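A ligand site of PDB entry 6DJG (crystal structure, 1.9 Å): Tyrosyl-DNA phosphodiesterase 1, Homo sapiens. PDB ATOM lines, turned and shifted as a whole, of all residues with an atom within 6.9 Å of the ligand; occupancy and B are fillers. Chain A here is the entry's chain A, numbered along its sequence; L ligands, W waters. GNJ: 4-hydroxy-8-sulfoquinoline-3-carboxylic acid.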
ATOM      1  N   ASN A  56      20.818 -25.861 -22.258  1.00  0.00           N
ATOM      2  CA  ASN A  56      19.629 -25.144 -21.829  1.00  0.00           C
ATOM      3  C   ASN A  56      19.519 -23.813 -22.552  1.00  0.00           C
ATOM      4  O   ASN A  56      20.284 -23.490 -23.457  1.00  0.00           O
ATOM      5  CB  ASN A  56      19.605 -24.949 -20.314  1.00  0.00           C
ATOM      6  CG  ASN A  56      18.218 -25.135 -19.742  1.00  0.00           C
ATOM      7  OD1 ASN A  56      17.333 -24.305 -19.961  1.00  0.00           O
ATOM      8  ND2 ASN A  56      18.000 -26.244 -19.031  1.00  0.00           N
ATOM      9  N   TYR A  57      18.504 -23.055 -22.150  1.00  0.00           N
ATOM     10  CA  TYR A  57      18.265 -21.731 -22.684  1.00  0.00           C
ATOM     11  C   TYR A  57      18.645 -20.674 -21.661  1.00  0.00           C
ATOM     12  O   TYR A  57      19.518 -19.827 -21.939  1.00  0.00           O
ATOM     13  CB  TYR A  57      16.782 -21.620 -23.080  1.00  0.00           C
ATOM     14  CG  TYR A  57      16.419 -20.239 -23.525  1.00  0.00           C
ATOM     15  CD1 TYR A  57      16.906 -19.734 -24.721  1.00  0.00           C
ATOM     16  CD2 TYR A  57      15.614 -19.423 -22.733  1.00  0.00           C
ATOM     17  CE1 TYR A  57      16.584 -18.443 -25.137  1.00  0.00           C
ATOM     18  CE2 TYR A  57      15.303 -18.128 -23.136  1.00  0.00           C
ATOM     19  CZ  TYR A  57      15.777 -17.657 -24.342  1.00  0.00           C
ATOM     20  OH  TYR A  57      15.452 -16.389 -24.747  1.00  0.00           O
ATOM     21  N   CYS A  58      18.062 -20.722 -20.472  1.00  0.00           N
ATOM     22  CA  CYS A  58      18.330 -19.747 -19.430  1.00  0.00           C
ATOM     23  C   CYS A  58      19.010 -20.438 -18.250  1.00  0.00           C
ATOM     24  O   CYS A  58      18.578 -21.507 -17.815  1.00  0.00           O
ATOM     25  CB  CYS A  58      17.026 -19.084 -18.968  1.00  0.00           C
ATOM     26  SG  CYS A  58      17.305 -17.714 -17.854  1.00  0.00           S
ATOM     27  N   THR A 114      16.967 -19.760 -31.670  1.00  0.00           N
ATOM     28  CA  THR A 114      17.322 -19.835 -30.263  1.00  0.00           C
ATOM     29  C   THR A 114      17.738 -21.265 -29.939  1.00  0.00           C
ATOM     30  O   THR A 114      17.499 -22.192 -30.717  1.00  0.00           O
ATOM     31  CB  THR A 114      16.155 -19.426 -29.357  1.00  0.00           C
ATOM     32  OG1 THR A 114      14.974 -20.070 -29.813  1.00  0.00           O
ATOM     33  CG2 THR A 114      15.939 -17.914 -29.364  1.00  0.00           C
ATOM     34  N   HIS A 115      18.377 -21.439 -28.783  1.00  0.00           N
ATOM     35  CA  HIS A 115      18.792 -22.775 -28.336  1.00  0.00           C
ATOM     36  C   HIS A 115      17.898 -23.169 -27.171  1.00  0.00           C
ATOM     37  O   HIS A 115      18.151 -22.790 -26.024  1.00  0.00           O
ATOM     38  CB  HIS A 115      20.263 -22.786 -27.918  1.00  0.00           C
ATOM     39  CG  HIS A 115      20.740 -24.135 -27.496  1.00  0.00           C
ATOM     40  ND1 HIS A 115      20.705 -24.553 -26.185  1.00  0.00           N
ATOM     41  CD2 HIS A 115      21.251 -25.172 -28.210  1.00  0.00           C
ATOM     42  CE1 HIS A 115      21.167 -25.787 -26.102  1.00  0.00           C
ATOM     43  NE2 HIS A 115      21.499 -26.194 -27.322  1.00  0.00           N
ATOM     44  N   HIS A 116      16.842 -23.934 -27.480  1.00  0.00           N
ATOM     45  CA  HIS A 116      15.835 -24.307 -26.485  1.00  0.00           C
ATOM     46  C   HIS A 116      16.030 -25.701 -25.894  1.00  0.00           C
ATOM     47  O   HIS A 116      15.390 -26.021 -24.888  1.00  0.00           O
ATOM     48  CB  HIS A 116      14.427 -24.242 -27.092  1.00  0.00           C
ATOM     49  CG  HIS A 116      13.941 -22.852 -27.350  1.00  0.00           C
ATOM     50  ND1 HIS A 116      13.064 -22.556 -28.366  1.00  0.00           N
ATOM     51  CD2 HIS A 116      14.203 -21.688 -26.712  1.00  0.00           C
ATOM     52  CE1 HIS A 116      12.797 -21.263 -28.345  1.00  0.00           C
ATOM     53  NE2 HIS A 116      13.476 -20.704 -27.353  1.00  0.00           N
ATOM     54  N   THR A 117      16.890 -26.510 -26.509  1.00  0.00           N
ATOM     55  CA  THR A 117      17.126 -27.882 -26.057  1.00  0.00           C
ATOM     56  C   THR A 117      17.496 -27.922 -24.583  1.00  0.00           C
ATOM     57  O   THR A 117      18.340 -27.151 -24.108  1.00  0.00           O
ATOM     58  CB  THR A 117      18.234 -28.519 -26.882  1.00  0.00           C
ATOM     59  OG1 THR A 117      17.744 -28.743 -28.210  1.00  0.00           O
ATOM     60  CG2 THR A 117      18.682 -29.847 -26.262  1.00  0.00           C
ATOM     61  N   LYS A 118      16.817 -28.792 -23.840  1.00  0.00           N
ATOM     62  CA  LYS A 118      17.058 -28.936 -22.415  1.00  0.00           C
ATOM     63  C   LYS A 118      17.437 -30.385 -22.147  1.00  0.00           C
ATOM     64  O   LYS A 118      16.615 -31.299 -22.283  1.00  0.00           O
ATOM     65  CB  LYS A 118      15.849 -28.455 -21.623  1.00  0.00           C
ATOM     66  CG  LYS A 118      15.702 -26.931 -21.844  1.00  0.00           C
ATOM     67  CD  LYS A 118      14.470 -26.366 -21.207  1.00  0.00           C
ATOM     68  CE  LYS A 118      14.379 -24.873 -21.508  1.00  0.00           C
ATOM     69  NZ  LYS A 118      13.948 -24.679 -22.919  1.00  0.00           N
ATOM     70  N   THR A 134      12.346 -30.278 -19.729  1.00  0.00           N
ATOM     71  CA  THR A 134      11.722 -29.069 -20.235  1.00  0.00           C
ATOM     72  C   THR A 134      12.025 -27.814 -19.424  1.00  0.00           C
ATOM     73  O   THR A 134      11.559 -26.731 -19.789  1.00  0.00           O
ATOM     74  CB  THR A 134      10.193 -29.262 -20.330  1.00  0.00           C
ATOM     75  OG1 THR A 134       9.627 -29.440 -19.025  1.00  0.00           O
ATOM     76  CG2 THR A 134       9.864 -30.481 -21.168  1.00  0.00           C
ATOM     77  N   SER A 135      12.814 -27.912 -18.366  1.00  0.00           N
ATOM     78  CA  SER A 135      13.027 -26.810 -17.426  1.00  0.00           C
ATOM     79  C   SER A 135      14.295 -26.030 -17.725  1.00  0.00           C
ATOM     80  O   SER A 135      15.354 -26.615 -17.984  1.00  0.00           O
ATOM     81  CB  SER A 135      13.109 -27.330 -15.990  1.00  0.00           C
ATOM     82  OG  SER A 135      11.967 -28.097 -15.678  1.00  0.00           O
ATOM     83  N   ASN A 136      14.196 -24.708 -17.613  1.00  0.00           N
ATOM     84  CA  ASN A 136      15.394 -23.882 -17.565  1.00  0.00           C
ATOM     85  C   ASN A 136      16.147 -24.121 -16.250  1.00  0.00           C
ATOM     86  O   ASN A 136      15.602 -24.658 -15.278  1.00  0.00           O
ATOM     87  CB  ASN A 136      15.034 -22.401 -17.702  1.00  0.00           C
ATOM     88  CG  ASN A 136      14.525 -22.067 -19.096  1.00  0.00           C
ATOM     89  OD1 ASN A 136      15.314 -21.841 -20.012  1.00  0.00           O
ATOM     90  ND2 ASN A 136      13.193 -22.037 -19.267  1.00  0.00           N
ATOM     91  N   ASP A 141      11.781 -22.284 -12.532  1.00  0.00           N
ATOM     92  CA  ASP A 141      11.316 -23.323 -13.433  1.00  0.00           C
ATOM     93  C   ASP A 141      11.139 -24.671 -12.737  1.00  0.00           C
ATOM     94  O   ASP A 141      10.449 -25.547 -13.274  1.00  0.00           O
ATOM     95  CB  ASP A 141      12.280 -23.470 -14.621  1.00  0.00           C
ATOM     96  CG  ASP A 141      11.808 -22.677 -15.832  1.00  0.00           C
ATOM     97  OD1 ASP A 141      11.254 -21.555 -15.637  1.00  0.00           O
ATOM     98  OD2 ASP A 141      11.961 -23.205 -16.952  1.00  0.00           O
ATOM     99  N   SER A 252       3.734 -23.993 -23.977  1.00  0.00           N
ATOM    100  CA  SER A 252       3.763 -22.800 -23.141  1.00  0.00           C
ATOM    101  C   SER A 252       4.061 -21.524 -23.910  1.00  0.00           C
ATOM    102  O   SER A 252       4.097 -20.447 -23.304  1.00  0.00           O
ATOM    103  CB  SER A 252       4.757 -22.970 -21.998  1.00  0.00           C
ATOM    104  OG  SER A 252       6.069 -23.205 -22.469  1.00  0.00           O
ATOM    105  N   SER A 253       4.308 -21.612 -25.222  1.00  0.00           N
ATOM    106  CA  SER A 253       4.456 -20.433 -26.078  1.00  0.00           C
ATOM    107  C   SER A 253       3.833 -20.762 -27.424  1.00  0.00           C
ATOM    108  O   SER A 253       3.772 -21.912 -27.832  1.00  0.00           O
ATOM    109  CB  SER A 253       5.918 -20.044 -26.313  1.00  0.00           C
ATOM    110  OG  SER A 253       6.646 -19.889 -25.107  1.00  0.00           O
ATOM    111  N   GLY A 310       2.799 -16.143 -15.657  1.00  0.00           N
ATOM    112  CA  GLY A 310       2.705 -15.639 -17.018  1.00  0.00           C
ATOM    113  C   GLY A 310       3.991 -15.067 -17.561  1.00  0.00           C
ATOM    114  O   GLY A 310       4.131 -14.926 -18.780  1.00  0.00           O
ATOM    115  N   GLY A 311       4.941 -14.730 -16.684  1.00  0.00           N
ATOM    116  CA  GLY A 311       6.281 -14.382 -17.110  1.00  0.00           C
ATOM    117  C   GLY A 311       6.955 -15.471 -17.927  1.00  0.00           C
ATOM    118  O   GLY A 311       7.855 -15.173 -18.718  1.00  0.00           O
ATOM    119  N   SER A 312       6.517 -16.722 -17.770  1.00  0.00           N
ATOM    120  CA  SER A 312       7.067 -17.851 -18.526  1.00  0.00           C
ATOM    121  C   SER A 312       6.088 -18.387 -19.561  1.00  0.00           C
ATOM    122  O   SER A 312       6.231 -19.539 -20.005  1.00  0.00           O
ATOM    123  CB  SER A 312       7.480 -18.972 -17.587  1.00  0.00           C
ATOM    124  OG  SER A 312       8.439 -18.520 -16.657  1.00  0.00           O
ATOM    125  N   LEU A 313       5.092 -17.587 -19.951  1.00  0.00           N
ATOM    126  CA  LEU A 313       4.133 -17.941 -21.005  1.00  0.00           C
ATOM    127  C   LEU A 313       4.125 -16.796 -22.004  1.00  0.00           C
ATOM    128  O   LEU A 313       3.198 -15.993 -22.047  1.00  0.00           O
ATOM    129  CB  LEU A 313       2.733 -18.182 -20.420  1.00  0.00           C
ATOM    130  CG  LEU A 313       2.567 -19.401 -19.492  1.00  0.00           C
ATOM    131  CD1 LEU A 313       1.380 -19.288 -18.514  1.00  0.00           C
ATOM    132  CD2 LEU A 313       2.434 -20.675 -20.324  1.00  0.00           C
ATOM    133  N   PRO A 314       5.176 -16.691 -22.833  1.00  0.00           N
ATOM    134  CA  PRO A 314       5.493 -15.421 -23.518  1.00  0.00           C
ATOM    135  C   PRO A 314       4.757 -15.244 -24.837  1.00  0.00           C
ATOM    136  O   PRO A 314       5.357 -15.047 -25.890  1.00  0.00           O
ATOM    137  CB  PRO A 314       7.005 -15.515 -23.691  1.00  0.00           C
ATOM    138  CG  PRO A 314       7.246 -16.978 -23.916  1.00  0.00           C
ATOM    139  CD  PRO A 314       6.238 -17.692 -23.020  1.00  0.00           C
ATOM    140  N   HIS A 346       5.168 -25.570 -18.090  1.00  0.00           N
ATOM    141  CA  HIS A 346       6.280 -25.251 -18.956  1.00  0.00           C
ATOM    142  C   HIS A 346       6.763 -26.488 -19.719  1.00  0.00           C
ATOM    143  O   HIS A 346       7.621 -26.374 -20.609  1.00  0.00           O
ATOM    144  CB  HIS A 346       7.414 -24.621 -18.130  1.00  0.00           C
ATOM    145  CG  HIS A 346       8.546 -24.066 -18.940  1.00  0.00           C
ATOM    146  ND1 HIS A 346       9.681 -24.793 -19.229  1.00  0.00           N
ATOM    147  CD2 HIS A 346       8.746 -22.838 -19.471  1.00  0.00           C
ATOM    148  CE1 HIS A 346      10.516 -24.046 -19.939  1.00  0.00           C
ATOM    149  NE2 HIS A 346       9.968 -22.854 -20.089  1.00  0.00           N
ATOM    150  N   LYS A 348       6.107 -29.279 -22.604  1.00  0.00           N
ATOM    151  CA  LYS A 348       5.405 -29.311 -23.883  1.00  0.00           C
ATOM    152  C   LYS A 348       5.228 -30.772 -24.244  1.00  0.00           C
ATOM    153  O   LYS A 348       6.159 -31.563 -24.109  1.00  0.00           O
ATOM    154  CB  LYS A 348       6.168 -28.608 -25.016  1.00  0.00           C
ATOM    155  CG  LYS A 348       6.431 -27.113 -24.759  1.00  0.00           C
ATOM    156  CD  LYS A 348       7.763 -26.902 -24.047  1.00  0.00           C
ATOM    157  CE  LYS A 348       8.061 -25.409 -23.934  1.00  0.00           C
ATOM    158  NZ  LYS A 348       8.701 -25.107 -22.646  1.00  0.00           N
ATOM    159  N   SER A 367      11.011 -29.850 -25.800  1.00  0.00           N
ATOM    160  CA  SER A 367      11.133 -28.411 -25.586  1.00  0.00           C
ATOM    161  C   SER A 367      10.365 -27.615 -26.636  1.00  0.00           C
ATOM    162  O   SER A 367      10.165 -26.407 -26.453  1.00  0.00           O
ATOM    163  CB  SER A 367      12.618 -28.008 -25.638  1.00  0.00           C
ATOM    164  OG  SER A 367      13.172 -28.303 -26.914  1.00  0.00           O
ATOM    165  N   ASN A 369       7.845 -25.671 -28.586  1.00  0.00           N
ATOM    166  CA  ASN A 369       6.539 -25.029 -28.476  1.00  0.00           C
ATOM    167  C   ASN A 369       5.809 -25.085 -29.820  1.00  0.00           C
ATOM    168  O   ASN A 369       6.302 -25.637 -30.803  1.00  0.00           O
ATOM    169  CB  ASN A 369       6.718 -23.592 -27.984  1.00  0.00           C
ATOM    170  CG  ASN A 369       6.805 -23.513 -26.493  1.00  0.00           C
ATOM    171  OD1 ASN A 369       5.969 -24.068 -25.785  1.00  0.00           O
ATOM    172  ND2 ASN A 369       7.840 -22.841 -25.992  1.00  0.00           N
ATOM    173  N   GLU A 391      15.945 -27.798 -30.669  1.00  0.00           N
ATOM    174  CA  GLU A 391      14.910 -28.367 -29.817  1.00  0.00           C
ATOM    175  C   GLU A 391      15.215 -29.848 -29.642  1.00  0.00           C
ATOM    176  O   GLU A 391      15.930 -30.455 -30.436  1.00  0.00           O
ATOM    177  CB  GLU A 391      13.501 -28.221 -30.424  1.00  0.00           C
ATOM    178  CG  GLU A 391      13.152 -26.840 -30.958  1.00  0.00           C
ATOM    179  CD  GLU A 391      12.752 -25.854 -29.863  1.00  0.00           C
ATOM    180  OE1 GLU A 391      12.715 -24.625 -30.150  1.00  0.00           O
ATOM    181  OE2 GLU A 391      12.485 -26.284 -28.726  1.00  0.00           O
ATOM    182  N   TRP A 443       1.164 -12.199 -22.406  1.00  0.00           N
ATOM    183  CA  TRP A 443       1.992 -11.776 -21.277  1.00  0.00           C
ATOM    184  C   TRP A 443       2.298 -10.292 -21.244  1.00  0.00           C
ATOM    185  O   TRP A 443       2.734  -9.807 -20.195  1.00  0.00           O
ATOM    186  CB  TRP A 443       3.314 -12.556 -21.234  1.00  0.00           C
ATOM    187  CG  TRP A 443       4.359 -12.165 -22.231  1.00  0.00           C
ATOM    188  CD1 TRP A 443       4.171 -11.669 -23.487  1.00  0.00           C
ATOM    189  CD2 TRP A 443       5.790 -12.291 -22.062  1.00  0.00           C
ATOM    190  NE1 TRP A 443       5.381 -11.453 -24.109  1.00  0.00           N
ATOM    191  CE2 TRP A 443       6.397 -11.833 -23.254  1.00  0.00           C
ATOM    192  CE3 TRP A 443       6.607 -12.736 -21.022  1.00  0.00           C
ATOM    193  CZ2 TRP A 443       7.779 -11.802 -23.429  1.00  0.00           C
ATOM    194  CZ3 TRP A 443       7.979 -12.700 -21.188  1.00  0.00           C
ATOM    195  CH2 TRP A 443       8.545 -12.253 -22.387  1.00  0.00           C
HETATM  196  C13 GNJ L   1      10.079 -15.704 -22.055  1.00  0.00           C
HETATM  197  C15 GNJ L   1       9.997 -17.832 -20.905  1.00  0.00           C
HETATM  198  C17 GNJ L   1      11.194 -19.748 -21.830  1.00  0.00           C
HETATM  199  C02 GNJ L   1      12.506 -21.695 -22.858  1.00  0.00           C
HETATM  200  C04 GNJ L   1      12.013 -20.246 -22.854  1.00  0.00           C
HETATM  201  C05 GNJ L   1      12.408 -19.393 -23.877  1.00  0.00           C
HETATM  202  C07 GNJ L   1      11.252 -17.619 -22.940  1.00  0.00           C
HETATM  203  C08 GNJ L   1      10.895 -16.267 -23.023  1.00  0.00           C
HETATM  204  C14 GNJ L   1       9.622 -16.493 -20.991  1.00  0.00           C
HETATM  205  C16 GNJ L   1      10.821 -18.400 -21.895  1.00  0.00           C
HETATM  206  N06 GNJ L   1      12.039 -18.116 -23.908  1.00  0.00           N
HETATM  207  O01 GNJ L   1      12.100 -22.529 -22.022  1.00  0.00           O
HETATM  208  O03 GNJ L   1      13.404 -22.023 -23.673  1.00  0.00           O
HETATM  209  O10 GNJ L   1      10.972 -15.851 -25.703  1.00  0.00           O
HETATM  210  O11 GNJ L   1      12.991 -15.158 -24.376  1.00  0.00           O
HETATM  211  O12 GNJ L   1      11.049 -13.827 -24.228  1.00  0.00           O
HETATM  212  O18 GNJ L   1      10.827 -20.452 -20.940  1.00  0.00           O
HETATM  213  S09 GNJ L   1      11.490 -15.261 -24.419  1.00  0.00           S
HETATM  214  O   HOH W   1      10.673 -19.982 -17.797  1.00  0.00           O
HETATM  215  O   HOH W   2      11.480 -24.767 -24.335  1.00  0.00           O
HETATM  216  O   HOH W   3      11.064 -22.232 -25.569  1.00  0.00           O
HETATM  217  O   HOH W   4      13.079 -18.025 -26.816  1.00  0.00           O
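A ring nitrogen (NE2) of His 346 is in hydrogen-bond range of an oxygen (O18) of the ligand, at 2.7 Å. The side-chain hydroxyl (OH) of Tyr 57 is in hydrogen-bond range of an oxygen (O11) of the ligand, at 2.8 Å. The side-chain amino group of Lys 118 is in salt-bridge range of an oxygen (O03) of the ligand, 2.8 Å away. An oxygen (O01) of the ligand lies within hydrogen-bond range of the side-chain amide nitrogen (ND2) of Asn 136, at 3.0 Å.
A ring nitrogen (NE2) of His 346 sits close to the side-chain amide nitrogen of Asn 136 (3.4 Å). The side-chain amino group of Lys 348 lies within hydrogen-bond range of the backbone carbonyl oxygen of His 346, at 2.6 Å. A ring nitrogen (ND1) of His 346 sits at hydrogen-bond distance from the backbone carbonyl oxygen of Thr 134 (2.8 Å). The backbone carbonyl oxygen (O) of His 116 sits at hydrogen-bond distance from the side-chain amino group (NZ) of Lys 118 (2.8 Å). OD2 of Asp 141 sits at hydrogen-bond distance from N of Asn 136, 2.8 Å away. The backbone NH (N) of Cys 58 is in hydrogen-bond range of the side-chain amide oxygen (OD1) of Asn 136 (3.0 Å). The side-chain amide oxygen (OD1) of Asn 136 sits close to the side-chain amide oxygen (OD1) of Asn 56 (3.2 Å). ND1 of His 116 sits at hydrogen-bond distance from OE1 of Glu 391 (2.8 Å).
Residues that only touch the ligand: His 116 (3.2 Å), Gly 311 (3.2 Å), Trp 443 (3.5 Å), Pro 314 (3.5 Å) and Ser 312 (3.8 Å). Hydrophobic or aromatic side chains within 4 Å of the ligand: Tyr 57, His 116, Pro 314, His 346 and Trp 443. Of the 25 residues printed, 9 come within 4 Å of the ligand.
Water W3 lies within hydrogen-bond range of O03 of the ligand (3.0 Å), ND2 of Asn 369 (3.3 Å) and NE2 of His 116 (3.4 Å). Water W4 bridges NE2 of His 116 and N06 of the ligand. Water W1 lies within hydrogen-bond range of OD1 of Asp 141 (2.7 Å), OG of Ser 312 (2.9 Å) and O18 of the ligand (3.2 Å). Water W2 lies within hydrogen-bond range of the side-chain amino group (NZ) of Lys 118 (2.8 Å), the backbone carbonyl oxygen (O) of Ser 367 (3.0 Å), the side-chain amino group (NZ) of Lys 348 (3.3 Å) and an oxygen (O01) of the ligand (3.3 Å).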
